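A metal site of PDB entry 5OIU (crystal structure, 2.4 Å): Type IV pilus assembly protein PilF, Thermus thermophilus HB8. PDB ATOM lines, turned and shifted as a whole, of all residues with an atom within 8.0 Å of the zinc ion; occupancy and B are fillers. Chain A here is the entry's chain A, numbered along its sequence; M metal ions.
The backbone carbonyl oxygen (O) of Cys 285 lies within hydrogen-bond range of the backbone NH (N) of Met 315.
N of Gly 322 is in hydrogen-bond range of O of Cys 317.
N of Gly 316 sits close to SG of Cys 285, 3.2 Å away.
O of Cys 320 lies within hydrogen-bond range of OG1 of Thr 323 (2.6 Å).
The side-chain sulfur (SG) of Cys 317 sits close to the backbone NH (N) of Arg 319 (3.4 Å).
The side-chain sulfur (SG) of Cys 282 lies close to the backbone NH (N) of His 284 (3.4 Å).
SG of Cys 320 lies close to N of Gly 324.
The backbone NH of Cys 282 sits at hydrogen-bond distance from the backbone carbonyl oxygen of Gly 324.
The nearest printed residue that does not touch the zinc ion is Gly 316 (4.2 Å).
The zinc ion is bound by the side-chain sulfur of Cys 285 (2.3 Å), the side-chain sulfur of Cys 320 (2.3 Å), the side-chain sulfur of Cys 317 (2.4 Å) and the side-chain sulfur of Cys 282 (2.4 Å).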
ATOM      1  N   VAL A 281      -8.899   2.276  21.964  1.00  0.00           N
ATOM      2  CA  VAL A 281      -8.186   3.341  22.643  1.00  0.00           C
ATOM      3  C   VAL A 281      -7.079   3.884  21.743  1.00  0.00           C
ATOM      4  O   VAL A 281      -6.318   3.122  21.121  1.00  0.00           O
ATOM      5  CB  VAL A 281      -7.605   2.858  23.985  1.00  0.00           C
ATOM      6  CG1 VAL A 281      -6.637   3.913  24.547  1.00  0.00           C
ATOM      7  CG2 VAL A 281      -8.757   2.556  24.970  1.00  0.00           C
ATOM      8  N   CYS A 282      -7.008   5.219  21.656  1.00  0.00           N
ATOM      9  CA  CYS A 282      -5.970   5.900  20.907  1.00  0.00           C
ATOM     10  C   CYS A 282      -4.583   5.481  21.395  1.00  0.00           C
ATOM     11  O   CYS A 282      -4.292   5.505  22.595  1.00  0.00           O
ATOM     12  CB  CYS A 282      -6.152   7.426  21.046  1.00  0.00           C
ATOM     13  SG  CYS A 282      -4.897   8.452  20.194  1.00  0.00           S
ATOM     14  N   GLU A 283      -3.740   5.082  20.462  1.00  0.00           N
ATOM     15  CA  GLU A 283      -2.401   4.658  20.852  1.00  0.00           C
ATOM     16  C   GLU A 283      -1.547   5.850  21.269  1.00  0.00           C
ATOM     17  O   GLU A 283      -0.639   5.692  22.084  1.00  0.00           O
ATOM     18  CB  GLU A 283      -1.740   3.883  19.707  1.00  0.00           C
ATOM     19  CG  GLU A 283      -2.331   2.486  19.512  1.00  0.00           C
ATOM     20  CD  GLU A 283      -2.065   1.540  20.694  1.00  0.00           C
ATOM     21  OE1 GLU A 283      -1.474   1.948  21.723  1.00  0.00           O
ATOM     22  OE2 GLU A 283      -2.438   0.360  20.592  1.00  0.00           O
ATOM     23  N   HIS A 284      -1.842   7.040  20.756  1.00  0.00           N
ATOM     24  CA  HIS A 284      -0.926   8.146  20.997  1.00  0.00           C
ATOM     25  C   HIS A 284      -1.124   8.770  22.367  1.00  0.00           C
ATOM     26  O   HIS A 284      -0.156   9.232  22.965  1.00  0.00           O
ATOM     27  CB  HIS A 284      -1.075   9.191  19.888  1.00  0.00           C
ATOM     28  CG  HIS A 284      -0.722   8.658  18.532  1.00  0.00           C
ATOM     29  ND1 HIS A 284       0.575   8.567  18.082  1.00  0.00           N
ATOM     30  CD2 HIS A 284      -1.495   8.130  17.556  1.00  0.00           C
ATOM     31  CE1 HIS A 284       0.592   8.054  16.874  1.00  0.00           C
ATOM     32  NE2 HIS A 284      -0.655   7.766  16.529  1.00  0.00           N
ATOM     33  N   CYS A 285      -2.339   8.772  22.888  1.00  0.00           N
ATOM     34  CA  CYS A 285      -2.596   9.393  24.187  1.00  0.00           C
ATOM     35  C   CYS A 285      -3.019   8.379  25.225  1.00  0.00           C
ATOM     36  O   CYS A 285      -3.641   8.747  26.225  1.00  0.00           O
ATOM     37  CB  CYS A 285      -3.630  10.508  24.047  1.00  0.00           C
ATOM     38  SG  CYS A 285      -5.226   9.937  23.498  1.00  0.00           S
ATOM     39  N   LYS A 286      -2.677   7.108  25.025  1.00  0.00           N
ATOM     40  CA  LYS A 286      -3.075   6.050  25.951  1.00  0.00           C
ATOM     41  C   LYS A 286      -2.350   6.195  27.271  1.00  0.00           C
ATOM     42  O   LYS A 286      -1.165   6.528  27.335  1.00  0.00           O
ATOM     43  CB  LYS A 286      -2.785   4.678  25.336  1.00  0.00           C
ATOM     44  CG  LYS A 286      -2.908   3.506  26.296  1.00  0.00           C
ATOM     45  CD  LYS A 286      -2.658   2.192  25.588  1.00  0.00           C
ATOM     46  CE  LYS A 286      -3.808   1.836  24.657  1.00  0.00           C
ATOM     47  NZ  LYS A 286      -3.369   0.905  23.556  1.00  0.00           N
ATOM     48  N   GLY A 314      -7.560   6.529  26.783  1.00  0.00           N
ATOM     49  CA  GLY A 314      -6.951   7.616  26.037  1.00  0.00           C
ATOM     50  C   GLY A 314      -7.303   8.937  26.693  1.00  0.00           C
ATOM     51  O   GLY A 314      -8.479   9.204  26.989  1.00  0.00           O
ATOM     52  N   MET A 315      -6.273   9.766  26.944  1.00  0.00           N
ATOM     53  CA  MET A 315      -6.499  11.096  27.509  1.00  0.00           C
ATOM     54  C   MET A 315      -7.311  11.948  26.560  1.00  0.00           C
ATOM     55  O   MET A 315      -8.142  12.752  26.999  1.00  0.00           O
ATOM     56  CB  MET A 315      -5.189  11.811  27.818  1.00  0.00           C
ATOM     57  CG  MET A 315      -4.309  11.162  28.827  1.00  0.00           C
ATOM     58  SD  MET A 315      -4.892  11.392  30.504  1.00  0.00           S
ATOM     59  CE  MET A 315      -5.172  13.154  30.532  1.00  0.00           C
ATOM     60  N   GLY A 316      -7.081  11.809  25.259  1.00  0.00           N
ATOM     61  CA  GLY A 316      -7.647  12.769  24.333  1.00  0.00           C
ATOM     62  C   GLY A 316      -6.579  13.699  23.800  1.00  0.00           C
ATOM     63  O   GLY A 316      -5.993  14.502  24.532  1.00  0.00           O
ATOM     64  N   CYS A 317      -6.317  13.597  22.502  1.00  0.00           N
ATOM     65  CA  CYS A 317      -5.232  14.306  21.874  1.00  0.00           C
ATOM     66  C   CYS A 317      -5.668  14.664  20.465  1.00  0.00           C
ATOM     67  O   CYS A 317      -6.789  14.336  20.048  1.00  0.00           O
ATOM     68  CB  CYS A 317      -3.946  13.456  21.900  1.00  0.00           C
ATOM     69  SG  CYS A 317      -3.872  12.151  20.683  1.00  0.00           S
ATOM     70  N   GLU A 318      -4.813  15.354  19.724  1.00  0.00           N
ATOM     71  CA  GLU A 318      -5.263  15.796  18.410  1.00  0.00           C
ATOM     72  C   GLU A 318      -5.426  14.622  17.465  1.00  0.00           C
ATOM     73  O   GLU A 318      -6.230  14.707  16.536  1.00  0.00           O
ATOM     74  CB  GLU A 318      -4.302  16.820  17.804  1.00  0.00           C
ATOM     75  CG  GLU A 318      -5.012  17.773  16.840  1.00  0.00           C
ATOM     76  CD  GLU A 318      -5.000  17.280  15.386  1.00  0.00           C
ATOM     77  OE1 GLU A 318      -4.282  16.306  15.080  1.00  0.00           O
ATOM     78  OE2 GLU A 318      -5.699  17.900  14.533  1.00  0.00           O
ATOM     79  N   ARG A 319      -4.678  13.539  17.671  1.00  0.00           N
ATOM     80  CA  ARG A 319      -4.735  12.422  16.742  1.00  0.00           C
ATOM     81  C   ARG A 319      -6.094  11.728  16.775  1.00  0.00           C
ATOM     82  O   ARG A 319      -6.503  11.153  15.766  1.00  0.00           O
ATOM     83  CB  ARG A 319      -3.614  11.429  17.039  1.00  0.00           C
ATOM     84  CG  ARG A 319      -2.221  12.028  16.902  1.00  0.00           C
ATOM     85  CD  ARG A 319      -1.857  12.257  15.429  1.00  0.00           C
ATOM     86  NE  ARG A 319      -1.082  11.132  14.907  1.00  0.00           N
ATOM     87  CZ  ARG A 319       0.251  11.052  14.960  1.00  0.00           C
ATOM     88  NH1 ARG A 319       0.962  12.030  15.502  1.00  0.00           N
ATOM     89  NH2 ARG A 319       0.868   9.989  14.459  1.00  0.00           N
ATOM     90  N   CYS A 320      -6.796  11.783  17.915  1.00  0.00           N
ATOM     91  CA  CYS A 320      -8.119  11.184  18.095  1.00  0.00           C
ATOM     92  C   CYS A 320      -9.217  12.220  18.247  1.00  0.00           C
ATOM     93  O   CYS A 320     -10.314  11.888  18.716  1.00  0.00           O
ATOM     94  CB  CYS A 320      -8.133  10.237  19.298  1.00  0.00           C
ATOM     95  SG  CYS A 320      -7.608  10.960  20.903  1.00  0.00           S
ATOM     96  N   GLY A 321      -8.967  13.465  17.868  1.00  0.00           N
ATOM     97  CA  GLY A 321      -9.958  14.509  18.055  1.00  0.00           C
ATOM     98  C   GLY A 321     -10.395  14.684  19.500  1.00  0.00           C
ATOM     99  O   GLY A 321     -11.566  14.972  19.750  1.00  0.00           O
ATOM    100  N   GLY A 322      -9.499  14.479  20.438  1.00  0.00           N
ATOM    101  CA  GLY A 322      -9.856  14.631  21.835  1.00  0.00           C
ATOM    102  C   GLY A 322     -10.817  13.607  22.365  1.00  0.00           C
ATOM    103  O   GLY A 322     -11.127  13.660  23.555  1.00  0.00           O
ATOM    104  N   THR A 323     -11.306  12.660  21.527  1.00  0.00           N
ATOM    105  CA  THR A 323     -12.216  11.618  21.983  1.00  0.00           C
ATOM    106  C   THR A 323     -11.557  10.573  22.863  1.00  0.00           C
ATOM    107  O   THR A 323     -12.246   9.913  23.639  1.00  0.00           O
ATOM    108  CB  THR A 323     -12.852  10.879  20.796  1.00  0.00           C
ATOM    109  OG1 THR A 323     -11.833  10.213  20.031  1.00  0.00           O
ATOM    110  CG2 THR A 323     -13.655  11.816  19.915  1.00  0.00           C
ATOM    111  N   GLY A 324     -10.246  10.366  22.732  1.00  0.00           N
ATOM    112  CA  GLY A 324      -9.574   9.244  23.372  1.00  0.00           C
ATOM    113  C   GLY A 324      -9.682   7.938  22.623  1.00  0.00           C
ATOM    114  O   GLY A 324      -9.265   6.897  23.140  1.00  0.00           O
ATOM    115  N   TYR A 325     -10.237   7.947  21.404  1.00  0.00           N
ATOM    116  CA  TYR A 325     -10.423   6.715  20.668  1.00  0.00           C
ATOM    117  C   TYR A 325     -10.116   6.934  19.195  1.00  0.00           C
ATOM    118  O   TYR A 325     -10.424   7.996  18.638  1.00  0.00           O
ATOM    119  CB  TYR A 325     -11.861   6.176  20.821  1.00  0.00           C
ATOM    120  CG  TYR A 325     -12.343   5.848  22.237  1.00  0.00           C
ATOM    121  CD1 TYR A 325     -12.062   4.605  22.843  1.00  0.00           C
ATOM    122  CD2 TYR A 325     -13.149   6.721  22.932  1.00  0.00           C
ATOM    123  CE1 TYR A 325     -12.545   4.276  24.125  1.00  0.00           C
ATOM    124  CE2 TYR A 325     -13.633   6.400  24.202  1.00  0.00           C
ATOM    125  CZ  TYR A 325     -13.331   5.188  24.792  1.00  0.00           C
ATOM    126  OH  TYR A 325     -13.838   4.914  26.052  1.00  0.00           O
ATOM    127  N   LYS A 326      -9.484   5.932  18.572  1.00  0.00           N
ATOM    128  CA  LYS A 326      -9.351   5.883  17.112  1.00  0.00           C
ATOM    129  C   LYS A 326      -9.615   4.468  16.646  1.00  0.00           C
ATOM    130  O   LYS A 326      -8.761   3.593  16.810  1.00  0.00           O
ATOM    131  CB  LYS A 326      -7.986   6.341  16.616  1.00  0.00           C
ATOM    132  CG  LYS A 326      -8.034   6.452  15.090  1.00  0.00           C
ATOM    133  CD  LYS A 326      -6.760   6.905  14.468  1.00  0.00           C
ATOM    134  CE  LYS A 326      -6.264   8.181  15.116  1.00  0.00           C
ATOM    135  NZ  LYS A 326      -5.036   7.986  15.991  1.00  0.00           N
HETATM  136 ZN    ZN M   1      -5.431  10.486  21.324  1.00  0.00          ZN
